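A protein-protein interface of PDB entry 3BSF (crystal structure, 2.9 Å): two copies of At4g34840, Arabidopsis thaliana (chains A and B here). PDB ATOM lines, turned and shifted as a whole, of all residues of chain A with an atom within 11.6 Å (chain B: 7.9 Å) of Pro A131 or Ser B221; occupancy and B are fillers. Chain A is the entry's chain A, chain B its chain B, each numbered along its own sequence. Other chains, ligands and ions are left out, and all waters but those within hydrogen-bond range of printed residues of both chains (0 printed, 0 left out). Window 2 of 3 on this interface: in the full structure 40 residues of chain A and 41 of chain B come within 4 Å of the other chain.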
ATOM      1  N   HIS A 126      12.501  14.439  -6.873  1.00  0.00           N
ATOM      2  CA  HIS A 126      12.426  13.017  -7.138  1.00  0.00           C
ATOM      3  C   HIS A 126      12.306  12.197  -5.843  1.00  0.00           C
ATOM      4  O   HIS A 126      12.100  10.975  -5.892  1.00  0.00           O
ATOM      5  CB  HIS A 126      13.644  12.558  -7.951  1.00  0.00           C
ATOM      6  CG  HIS A 126      14.956  12.685  -7.227  1.00  0.00           C
ATOM      7  ND1 HIS A 126      16.000  13.450  -7.708  1.00  0.00           N
ATOM      8  CD2 HIS A 126      15.408  12.110  -6.087  1.00  0.00           C
ATOM      9  CE1 HIS A 126      17.035  13.337  -6.897  1.00  0.00           C
ATOM     10  NE2 HIS A 126      16.703  12.530  -5.906  1.00  0.00           N
ATOM     11  N   ASP A 127      12.411  12.868  -4.691  1.00  0.00           N
ATOM     12  CA  ASP A 127      12.318  12.189  -3.389  1.00  0.00           C
ATOM     13  C   ASP A 127      11.138  12.588  -2.483  1.00  0.00           C
ATOM     14  O   ASP A 127      11.230  12.436  -1.268  1.00  0.00           O
ATOM     15  CB  ASP A 127      13.647  12.339  -2.611  1.00  0.00           C
ATOM     16  CG  ASP A 127      13.837  13.733  -1.978  1.00  0.00           C
ATOM     17  OD1 ASP A 127      13.551  14.756  -2.649  1.00  0.00           O
ATOM     18  OD2 ASP A 127      14.303  13.803  -0.806  1.00  0.00           O
ATOM     19  N   ARG A 128      10.047  13.094  -3.070  1.00  0.00           N
ATOM     20  CA  ARG A 128       8.847  13.493  -2.305  1.00  0.00           C
ATOM     21  C   ARG A 128       7.641  12.757  -2.879  1.00  0.00           C
ATOM     22  O   ARG A 128       6.724  13.349  -3.450  1.00  0.00           O
ATOM     23  CB  ARG A 128       8.593  15.011  -2.367  1.00  0.00           C
ATOM     24  CG  ARG A 128       9.783  15.870  -1.962  1.00  0.00           C
ATOM     25  CD  ARG A 128       9.366  17.282  -1.579  1.00  0.00           C
ATOM     26  NE  ARG A 128       8.525  17.954  -2.570  1.00  0.00           N
ATOM     27  CZ  ARG A 128       7.959  19.147  -2.376  1.00  0.00           C
ATOM     28  NH1 ARG A 128       8.158  19.793  -1.225  1.00  0.00           N
ATOM     29  NH2 ARG A 128       7.174  19.675  -3.317  1.00  0.00           N
ATOM     30  N   ARG A 129       7.664  11.445  -2.697  1.00  0.00           N
ATOM     31  CA  ARG A 129       6.629  10.555  -3.185  1.00  0.00           C
ATOM     32  C   ARG A 129       5.396  10.470  -2.281  1.00  0.00           C
ATOM     33  O   ARG A 129       5.415   9.806  -1.256  1.00  0.00           O
ATOM     34  CB  ARG A 129       7.242   9.165  -3.379  1.00  0.00           C
ATOM     35  CG  ARG A 129       8.584   9.172  -4.130  1.00  0.00           C
ATOM     36  CD  ARG A 129       9.191   7.774  -4.168  1.00  0.00           C
ATOM     37  NE  ARG A 129       9.377   7.237  -2.820  1.00  0.00           N
ATOM     38  CZ  ARG A 129      10.472   7.415  -2.088  1.00  0.00           C
ATOM     39  NH1 ARG A 129      11.494   8.112  -2.577  1.00  0.00           N
ATOM     40  NH2 ARG A 129      10.529   6.910  -0.863  1.00  0.00           N
ATOM     41  N   ILE A 130       4.322  11.146  -2.669  1.00  0.00           N
ATOM     42  CA  ILE A 130       3.093  11.124  -1.888  1.00  0.00           C
ATOM     43  C   ILE A 130       2.023  10.451  -2.740  1.00  0.00           C
ATOM     44  O   ILE A 130       1.424  11.085  -3.606  1.00  0.00           O
ATOM     45  CB  ILE A 130       2.633  12.537  -1.555  1.00  0.00           C
ATOM     46  CG1 ILE A 130       3.826  13.378  -1.095  1.00  0.00           C
ATOM     47  CG2 ILE A 130       1.588  12.481  -0.466  1.00  0.00           C
ATOM     48  CD1 ILE A 130       3.481  14.820  -0.842  1.00  0.00           C
ATOM     49  N   PRO A 131       1.773   9.148  -2.507  1.00  0.00           N
ATOM     50  CA  PRO A 131       0.787   8.324  -3.229  1.00  0.00           C
ATOM     51  C   PRO A 131      -0.670   8.771  -3.081  1.00  0.00           C
ATOM     52  O   PRO A 131      -1.526   8.006  -2.642  1.00  0.00           O
ATOM     53  CB  PRO A 131       1.020   6.931  -2.653  1.00  0.00           C
ATOM     54  CG  PRO A 131       1.401   7.225  -1.223  1.00  0.00           C
ATOM     55  CD  PRO A 131       2.366   8.394  -1.384  1.00  0.00           C
ATOM     56  N   VAL A 132      -0.942  10.012  -3.466  1.00  0.00           N
ATOM     57  CA  VAL A 132      -2.277  10.582  -3.373  1.00  0.00           C
ATOM     58  C   VAL A 132      -2.601  11.350  -4.655  1.00  0.00           C
ATOM     59  O   VAL A 132      -1.711  11.928  -5.285  1.00  0.00           O
ATOM     60  CB  VAL A 132      -2.360  11.511  -2.138  1.00  0.00           C
ATOM     61  CG1 VAL A 132      -3.543  12.433  -2.230  1.00  0.00           C
ATOM     62  CG2 VAL A 132      -2.472  10.672  -0.885  1.00  0.00           C
ATOM     63  N   PRO A 133      -3.878  11.341  -5.073  1.00  0.00           N
ATOM     64  CA  PRO A 133      -4.398  12.010  -6.270  1.00  0.00           C
ATOM     65  C   PRO A 133      -3.709  13.296  -6.755  1.00  0.00           C
ATOM     66  O   PRO A 133      -3.074  13.279  -7.812  1.00  0.00           O
ATOM     67  CB  PRO A 133      -5.860  12.216  -5.916  1.00  0.00           C
ATOM     68  CG  PRO A 133      -6.180  10.893  -5.264  1.00  0.00           C
ATOM     69  CD  PRO A 133      -4.962  10.609  -4.384  1.00  0.00           C
ATOM     70  N   VAL A 134      -3.828  14.405  -6.019  1.00  0.00           N
ATOM     71  CA  VAL A 134      -3.185  15.648  -6.469  1.00  0.00           C
ATOM     72  C   VAL A 134      -1.882  15.930  -5.729  1.00  0.00           C
ATOM     73  O   VAL A 134      -0.987  16.614  -6.246  1.00  0.00           O
ATOM     74  CB  VAL A 134      -4.121  16.885  -6.315  1.00  0.00           C
ATOM     75  CG1 VAL A 134      -4.490  17.094  -4.851  1.00  0.00           C
ATOM     76  CG2 VAL A 134      -3.432  18.128  -6.845  1.00  0.00           C
ATOM     77  N   LEU A 135      -1.784  15.389  -4.519  1.00  0.00           N
ATOM     78  CA  LEU A 135      -0.596  15.559  -3.688  1.00  0.00           C
ATOM     79  C   LEU A 135       0.672  14.975  -4.285  1.00  0.00           C
ATOM     80  O   LEU A 135       1.763  15.396  -3.936  1.00  0.00           O
ATOM     81  CB  LEU A 135      -0.830  14.947  -2.309  1.00  0.00           C
ATOM     82  CG  LEU A 135      -1.551  15.902  -1.368  1.00  0.00           C
ATOM     83  CD1 LEU A 135      -2.393  15.130  -0.363  1.00  0.00           C
ATOM     84  CD2 LEU A 135      -0.513  16.789  -0.702  1.00  0.00           C
ATOM     85  N   ASP A 136       0.539  14.001  -5.171  1.00  0.00           N
ATOM     86  CA  ASP A 136       1.722  13.410  -5.780  1.00  0.00           C
ATOM     87  C   ASP A 136       2.347  14.348  -6.815  1.00  0.00           C
ATOM     88  O   ASP A 136       3.546  14.275  -7.073  1.00  0.00           O
ATOM     89  CB  ASP A 136       1.388  12.044  -6.401  1.00  0.00           C
ATOM     90  CG  ASP A 136       0.414  12.137  -7.554  1.00  0.00           C
ATOM     91  OD1 ASP A 136      -0.631  12.803  -7.409  1.00  0.00           O
ATOM     92  OD2 ASP A 136       0.695  11.526  -8.608  1.00  0.00           O
ATOM     93  N   ILE A 137       1.530  15.235  -7.389  1.00  0.00           N
ATOM     94  CA  ILE A 137       2.003  16.214  -8.369  1.00  0.00           C
ATOM     95  C   ILE A 137       2.702  17.314  -7.594  1.00  0.00           C
ATOM     96  O   ILE A 137       3.709  17.878  -8.035  1.00  0.00           O
ATOM     97  CB  ILE A 137       0.835  16.809  -9.179  1.00  0.00           C
ATOM     98  CG1 ILE A 137       0.480  15.872 -10.338  1.00  0.00           C
ATOM     99  CG2 ILE A 137       1.223  18.158  -9.744  1.00  0.00           C
ATOM    100  CD1 ILE A 137       0.109  14.472  -9.921  1.00  0.00           C
ATOM    101  N   TYR A 138       2.149  17.617  -6.427  1.00  0.00           N
ATOM    102  CA  TYR A 138       2.723  18.617  -5.554  1.00  0.00           C
ATOM    103  C   TYR A 138       4.105  18.103  -5.168  1.00  0.00           C
ATOM    104  O   TYR A 138       5.093  18.837  -5.199  1.00  0.00           O
ATOM    105  CB  TYR A 138       1.846  18.775  -4.302  1.00  0.00           C
ATOM    106  CG  TYR A 138       2.470  19.605  -3.206  1.00  0.00           C
ATOM    107  CD1 TYR A 138       2.734  20.960  -3.391  1.00  0.00           C
ATOM    108  CD2 TYR A 138       2.813  19.024  -1.988  1.00  0.00           C
ATOM    109  CE1 TYR A 138       3.322  21.714  -2.393  1.00  0.00           C
ATOM    110  CE2 TYR A 138       3.402  19.770  -0.979  1.00  0.00           C
ATOM    111  CZ  TYR A 138       3.657  21.114  -1.184  1.00  0.00           C
ATOM    112  OH  TYR A 138       4.250  21.848  -0.174  1.00  0.00           O
ATOM    113  N   GLY A 139       4.150  16.821  -4.819  1.00  0.00           N
ATOM    114  CA  GLY A 139       5.387  16.178  -4.412  1.00  0.00           C
ATOM    115  C   GLY A 139       6.501  16.382  -5.415  1.00  0.00           C
ATOM    116  O   GLY A 139       7.620  16.788  -5.069  1.00  0.00           O
ATOM    117  N   VAL A 140       6.195  16.075  -6.668  1.00  0.00           N
ATOM    118  CA  VAL A 140       7.154  16.258  -7.748  1.00  0.00           C
ATOM    119  C   VAL A 140       7.405  17.758  -7.870  1.00  0.00           C
ATOM    120  O   VAL A 140       8.519  18.186  -8.184  1.00  0.00           O
ATOM    121  CB  VAL A 140       6.594  15.748  -9.087  1.00  0.00           C
ATOM    122  CG1 VAL A 140       7.632  15.902 -10.184  1.00  0.00           C
ATOM    123  CG2 VAL A 140       6.161  14.322  -8.937  1.00  0.00           C
ATOM    124  N   HIS A 173      14.167   3.757  -5.834  1.00  0.00           N
ATOM    125  CA  HIS A 173      12.990   4.630  -5.834  1.00  0.00           C
ATOM    126  C   HIS A 173      13.329   6.011  -6.407  1.00  0.00           C
ATOM    127  O   HIS A 173      12.527   6.624  -7.107  1.00  0.00           O
ATOM    128  CB  HIS A 173      12.463   4.815  -4.410  1.00  0.00           C
ATOM    129  CG  HIS A 173      11.301   3.937  -4.076  1.00  0.00           C
ATOM    130  ND1 HIS A 173      11.409   2.568  -3.951  1.00  0.00           N
ATOM    131  CD2 HIS A 173      10.000   4.235  -3.847  1.00  0.00           C
ATOM    132  CE1 HIS A 173      10.224   2.062  -3.661  1.00  0.00           C
ATOM    133  NE2 HIS A 173       9.352   3.051  -3.592  1.00  0.00           N
ATOM    134  N   GLU A 176      13.776   5.601 -10.346  1.00  0.00           N
ATOM    135  CA  GLU A 176      12.544   5.568 -11.134  1.00  0.00           C
ATOM    136  C   GLU A 176      11.924   6.969 -11.300  1.00  0.00           C
ATOM    137  O   GLU A 176      11.436   7.302 -12.384  1.00  0.00           O
ATOM    138  CB  GLU A 176      11.512   4.626 -10.499  1.00  0.00           C
ATOM    139  CG  GLU A 176      11.176   4.953  -9.037  1.00  0.00           C
ATOM    140  CD  GLU A 176       9.674   5.179  -8.755  1.00  0.00           C
ATOM    141  OE1 GLU A 176       8.864   4.267  -9.065  1.00  0.00           O
ATOM    142  OE2 GLU A 176       9.308   6.263  -8.206  1.00  0.00           O
ATOM    143  N   SER A 177      11.940   7.781 -10.235  1.00  0.00           N
ATOM    144  CA  SER A 177      11.376   9.131 -10.284  1.00  0.00           C
ATOM    145  C   SER A 177      12.232  10.068 -11.126  1.00  0.00           C
ATOM    146  O   SER A 177      11.701  10.841 -11.921  1.00  0.00           O
ATOM    147  CB  SER A 177      11.220   9.712  -8.878  1.00  0.00           C
ATOM    148  OG  SER A 177      10.313   8.936  -8.113  1.00  0.00           O
ATOM    149  N   ASP B 166      10.129  13.416   3.324  1.00  0.00           N
ATOM    150  CA  ASP B 166       9.228  14.042   2.360  1.00  0.00           C
ATOM    151  C   ASP B 166       8.314  13.091   1.586  1.00  0.00           C
ATOM    152  O   ASP B 166       7.550  13.516   0.726  1.00  0.00           O
ATOM    153  CB  ASP B 166      10.037  14.905   1.381  1.00  0.00           C
ATOM    154  CG  ASP B 166      10.544  16.180   2.020  1.00  0.00           C
ATOM    155  OD1 ASP B 166       9.693  17.012   2.399  1.00  0.00           O
ATOM    156  OD2 ASP B 166      11.784  16.341   2.145  1.00  0.00           O
ATOM    157  N   SER B 167       8.381  11.803   1.882  1.00  0.00           N
ATOM    158  CA  SER B 167       7.525  10.862   1.179  1.00  0.00           C
ATOM    159  C   SER B 167       6.537  10.273   2.152  1.00  0.00           C
ATOM    160  O   SER B 167       6.870  10.017   3.307  1.00  0.00           O
ATOM    161  CB  SER B 167       8.340   9.735   0.539  1.00  0.00           C
ATOM    162  OG  SER B 167       9.242  10.228  -0.431  1.00  0.00           O
ATOM    163  N   MET B 168       5.315  10.074   1.681  1.00  0.00           N
ATOM    164  CA  MET B 168       4.283   9.497   2.519  1.00  0.00           C
ATOM    165  C   MET B 168       4.411   7.975   2.473  1.00  0.00           C
ATOM    166  O   MET B 168       4.037   7.280   3.424  1.00  0.00           O
ATOM    167  CB  MET B 168       2.900   9.928   2.044  1.00  0.00           C
ATOM    168  CG  MET B 168       1.809   9.505   3.002  1.00  0.00           C
ATOM    169  SD  MET B 168       0.163  10.104   2.593  1.00  0.00           S
ATOM    170  CE  MET B 168      -0.398   8.817   1.374  1.00  0.00           C
ATOM    171  N   ASP B 169       4.943   7.451   1.372  1.00  0.00           N
ATOM    172  CA  ASP B 169       5.131   6.019   1.286  1.00  0.00           C
ATOM    173  C   ASP B 169       6.382   5.725   2.114  1.00  0.00           C
ATOM    174  O   ASP B 169       6.775   6.525   2.975  1.00  0.00           O
ATOM    175  CB  ASP B 169       5.327   5.576  -0.167  1.00  0.00           C
ATOM    176  CG  ASP B 169       6.594   6.147  -0.809  1.00  0.00           C
ATOM    177  OD1 ASP B 169       7.597   6.416  -0.107  1.00  0.00           O
ATOM    178  OD2 ASP B 169       6.593   6.301  -2.050  1.00  0.00           O
ATOM    179  N   MET B 170       7.009   4.584   1.858  1.00  0.00           N
ATOM    180  CA  MET B 170       8.227   4.206   2.569  1.00  0.00           C
ATOM    181  C   MET B 170       9.049   3.202   1.762  1.00  0.00           C
ATOM    182  O   MET B 170       8.698   2.030   1.686  1.00  0.00           O
ATOM    183  CB  MET B 170       7.876   3.604   3.930  1.00  0.00           C
ATOM    184  CG  MET B 170       9.076   3.073   4.698  1.00  0.00           C
ATOM    185  SD  MET B 170       8.680   2.621   6.403  1.00  0.00           S
ATOM    186  CE  MET B 170       8.262   0.903   6.240  1.00  0.00           C
ATOM    187  N   MET B 188       6.092  13.894   7.937  1.00  0.00           N
ATOM    188  CA  MET B 188       6.743  14.660   6.879  1.00  0.00           C
ATOM    189  C   MET B 188       7.275  16.060   7.196  1.00  0.00           C
ATOM    190  O   MET B 188       7.759  16.747   6.293  1.00  0.00           O
ATOM    191  CB  MET B 188       5.789  14.779   5.697  1.00  0.00           C
ATOM    192  CG  MET B 188       5.287  13.456   5.141  1.00  0.00           C
ATOM    193  SD  MET B 188       4.133  13.708   3.750  1.00  0.00           S
ATOM    194  CE  MET B 188       5.294  14.206   2.441  1.00  0.00           C
ATOM    195  N   ASP B 212      -2.195   5.982  10.876  1.00  0.00           N
ATOM    196  CA  ASP B 212      -1.915   4.841  10.027  1.00  0.00           C
ATOM    197  C   ASP B 212      -0.793   3.984  10.605  1.00  0.00           C
ATOM    198  O   ASP B 212       0.226   4.501  11.057  1.00  0.00           O
ATOM    199  CB  ASP B 212      -1.539   5.362   8.633  1.00  0.00           C
ATOM    200  CG  ASP B 212      -0.926   4.295   7.744  1.00  0.00           C
ATOM    201  OD1 ASP B 212      -1.543   3.212   7.591  1.00  0.00           O
ATOM    202  OD2 ASP B 212       0.175   4.543   7.190  1.00  0.00           O
ATOM    203  N   ARG B 218      -3.314  -3.336   6.544  1.00  0.00           N
ATOM    204  CA  ARG B 218      -4.081  -2.305   5.851  1.00  0.00           C
ATOM    205  C   ARG B 218      -3.123  -1.221   5.351  1.00  0.00           C
ATOM    206  O   ARG B 218      -2.287  -0.731   6.108  1.00  0.00           O
ATOM    207  CB  ARG B 218      -5.099  -1.694   6.812  1.00  0.00           C
ATOM    208  CG  ARG B 218      -6.140  -0.800   6.165  1.00  0.00           C
ATOM    209  CD  ARG B 218      -7.209  -1.607   5.452  1.00  0.00           C
ATOM    210  NE  ARG B 218      -8.395  -0.794   5.191  1.00  0.00           N
ATOM    211  CZ  ARG B 218      -8.417   0.260   4.384  1.00  0.00           C
ATOM    212  NH1 ARG B 218      -7.314   0.631   3.750  1.00  0.00           N
ATOM    213  NH2 ARG B 218      -9.538   0.949   4.215  1.00  0.00           N
ATOM    214  N   PRO B 219      -3.238  -0.836   4.069  1.00  0.00           N
ATOM    215  CA  PRO B 219      -2.436   0.177   3.356  1.00  0.00           C
ATOM    216  C   PRO B 219      -2.149   1.496   4.097  1.00  0.00           C
ATOM    217  O   PRO B 219      -2.752   1.773   5.133  1.00  0.00           O
ATOM    218  CB  PRO B 219      -3.240   0.397   2.081  1.00  0.00           C
ATOM    219  CG  PRO B 219      -3.789  -0.969   1.819  1.00  0.00           C
ATOM    220  CD  PRO B 219      -4.275  -1.392   3.183  1.00  0.00           C
ATOM    221  N   THR B 220      -1.233   2.306   3.553  1.00  0.00           N
ATOM    222  CA  THR B 220      -0.864   3.593   4.166  1.00  0.00           C
ATOM    223  C   THR B 220      -1.703   4.790   3.695  1.00  0.00           C
ATOM    224  O   THR B 220      -1.628   5.876   4.273  1.00  0.00           O
ATOM    225  CB  THR B 220       0.649   3.949   3.929  1.00  0.00           C
ATOM    226  OG1 THR B 220       0.912   4.082   2.523  1.00  0.00           O
ATOM    227  CG2 THR B 220       1.560   2.880   4.530  1.00  0.00           C
ATOM    228  N   SER B 221      -2.512   4.594   2.662  1.00  0.00           N
ATOM    229  CA  SER B 221      -3.318   5.690   2.146  1.00  0.00           C
ATOM    230  C   SER B 221      -4.808   5.648   2.480  1.00  0.00           C
ATOM    231  O   SER B 221      -5.417   6.702   2.655  1.00  0.00           O
ATOM    232  CB  SER B 221      -3.127   5.794   0.634  1.00  0.00           C
ATOM    233  OG  SER B 221      -1.761   6.013   0.333  1.00  0.00           O
ATOM    234  N   GLU B 222      -5.398   4.455   2.573  1.00  0.00           N
ATOM    235  CA  GLU B 222      -6.825   4.358   2.886  1.00  0.00           C
ATOM    236  C   GLU B 222      -7.092   4.328   4.385  1.00  0.00           C
ATOM    237  O   GLU B 222      -8.140   4.781   4.846  1.00  0.00           O
ATOM    238  CB  GLU B 222      -7.459   3.119   2.252  1.00  0.00           C
ATOM    239  CG  GLU B 222      -7.075   2.886   0.817  1.00  0.00           C
ATOM    240  CD  GLU B 222      -5.897   1.948   0.704  1.00  0.00           C
ATOM    241  OE1 GLU B 222      -6.069   0.757   1.033  1.00  0.00           O
ATOM    242  OE2 GLU B 222      -4.802   2.396   0.300  1.00  0.00           O
ATOM    243  N   GLU B 223      -6.153   3.780   5.147  1.00  0.00           N
ATOM    244  CA  GLU B 223      -6.309   3.719   6.597  1.00  0.00           C
ATOM    245  C   GLU B 223      -6.147   5.141   7.149  1.00  0.00           C
ATOM    246  O   GLU B 223      -6.744   5.503   8.168  1.00  0.00           O
ATOM    247  CB  GLU B 223      -5.254   2.775   7.194  1.00  0.00           C
ATOM    248  CG  GLU B 223      -5.425   2.471   8.684  1.00  0.00           C
ATOM    249  CD  GLU B 223      -4.472   1.391   9.181  1.00  0.00           C
ATOM    250  OE1 GLU B 223      -3.237   1.576   9.080  1.00  0.00           O
ATOM    251  OE2 GLU B 223      -4.960   0.353   9.676  1.00  0.00           O
ATOM    252  N   PHE B 224      -5.339   5.936   6.445  1.00  0.00           N
ATOM    253  CA  PHE B 224      -5.068   7.329   6.796  1.00  0.00           C
ATOM    254  C   PHE B 224      -6.320   8.179   6.639  1.00  0.00           C
ATOM    255  O   PHE B 224      -6.632   8.994   7.507  1.00  0.00           O
ATOM    256  CB  PHE B 224      -3.947   7.893   5.900  1.00  0.00           C
ATOM    257  CG  PHE B 224      -3.853   9.412   5.899  1.00  0.00           C
ATOM    258  CD1 PHE B 224      -3.590  10.118   7.076  1.00  0.00           C
ATOM    259  CD2 PHE B 224      -4.018  10.133   4.713  1.00  0.00           C
ATOM    260  CE1 PHE B 224      -3.491  11.516   7.072  1.00  0.00           C
ATOM    261  CE2 PHE B 224      -3.921  11.532   4.700  1.00  0.00           C
ATOM    262  CZ  PHE B 224      -3.658  12.221   5.882  1.00  0.00           C
ATOM    263  N   LEU B 225      -7.040   7.982   5.534  1.00  0.00           N
ATOM    264  CA  LEU B 225      -8.250   8.757   5.251  1.00  0.00           C
ATOM    265  C   LEU B 225      -9.479   8.446   6.123  1.00  0.00           C
ATOM    266  O   LEU B 225     -10.153   9.367   6.582  1.00  0.00           O
ATOM    267  CB  LEU B 225      -8.616   8.637   3.758  1.00  0.00           C
ATOM    268  CG  LEU B 225      -7.601   9.170   2.733  1.00  0.00           C
ATOM    269  CD1 LEU B 225      -8.148   8.997   1.321  1.00  0.00           C
ATOM    270  CD2 LEU B 225      -7.309  10.638   3.007  1.00  0.00           C
ATOM    271  N   GLU B 226      -9.778   7.173   6.368  1.00  0.00           N
ATOM    272  CA  GLU B 226     -10.945   6.835   7.185  1.00  0.00           C
ATOM    273  C   GLU B 226     -10.754   7.172   8.662  1.00  0.00           C
ATOM    274  O   GLU B 226     -11.676   7.025   9.469  1.00  0.00           O
ATOM    275  CB  GLU B 226     -11.286   5.354   7.024  1.00  0.00           C
ATOM    276  CG  GLU B 226     -10.090   4.431   7.130  1.00  0.00           C
ATOM    277  CD  GLU B 226     -10.428   3.006   6.754  1.00  0.00           C
ATOM    278  OE1 GLU B 226     -10.976   2.794   5.648  1.00  0.00           O
ATOM    279  OE2 GLU B 226     -10.137   2.103   7.565  1.00  0.00           O
ATOM    280  N   ASN B 227      -9.556   7.638   9.002  1.00  0.00           N
ATOM    281  CA  ASN B 227      -9.221   8.001  10.379  1.00  0.00           C
ATOM    282  C   ASN B 227      -8.790   9.468  10.582  1.00  0.00           C
ATOM    283  O   ASN B 227      -8.759   9.939  11.721  1.00  0.00           O
ATOM    284  CB  ASN B 227      -8.128   7.065  10.918  1.00  0.00           C
ATOM    285  CG  ASN B 227      -8.621   5.647  11.125  1.00  0.00           C
ATOM    286  OD1 ASN B 227      -9.200   5.040  10.225  1.00  0.00           O
ATOM    287  ND2 ASN B 227      -8.386   5.111  12.313  1.00  0.00           N
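N of Arg A129 lies within hydrogen-bond range of OG of Ser B167, 3.0 Å away.
The backbone carbonyl oxygen of Asp A127 lies within hydrogen-bond range of the side-chain hydroxyl of Ser B167 (3.1 Å).
The backbone NH (N) of Met B168 sits at hydrogen-bond distance from the backbone carbonyl oxygen (O) of Arg A129 (3.0 Å).
The guanidinium group (NE) of Arg A129 is in salt-bridge range of the side-chain carboxylate (OD2) of Asp B169, at 3.0 Å.
O of Tyr A138 is in hydrogen-bond range of NH2 of Arg A128 (2.9 Å).
O of Gly A139 is in hydrogen-bond range of NE of Arg A128 (2.9 Å).
The side-chain carboxylate of Asp A136 sits close to the backbone carbonyl oxygen of Val A132 (2.5 Å).
The backbone NH (N) of Asp A136 sits close to the backbone carbonyl oxygen (O) of Ile A130, 3.4 Å away.
Among the printed residues, merely in contact across the chains: Arg A128 with Asp B166, Pro A131 with Met B168, Val A132 with Met B168, Pro A131 with Ser B221, Arg A128 with Ser B167, Ile A130 with Met B188, Asp A127 with Asp B166, Ile A130 with Met B168 and Pro A131 with Asp B169.
Of the printed residues of chain B, Arg A129 touches Ser B167, Met B168 and Asp B169.
Of the printed residues of chain B, Ile A130 touches Met B168 (3.8 Å) and Met B188 (3.8 Å).
Pro A131 touches just these residues of chain B: Met B168 (3.5 Å), Asp B169 (3.9 Å) and Ser B221 (3.6 Å).
Met B168 touches four residues of chain A.
No residue of chain A comes within 4 Å of Pro B219.
Ser B221 touches just one residue of chain A: Pro A131.
No residue of chain A comes within 4 Å of Glu B222.
No residue of chain A comes within 4 Å of Leu B225.
Of the 17 printed residues of chain B, 6 touch a printed residue of chain A.
Hydrophobic or aromatic side chains of chain A within 4 Å of the printed part of chain B: Ile A130, Pro A131 and Val A132.
Among the printed residues, 13 pairs touch across the chains.
Among the printed residues, Asp or Glu carboxylates within 4 Å of a Lys or Arg side-chain nitrogen of the other chain: Arg A129 with Asp B169 (3.0 Å).
No position is printed for both chains.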
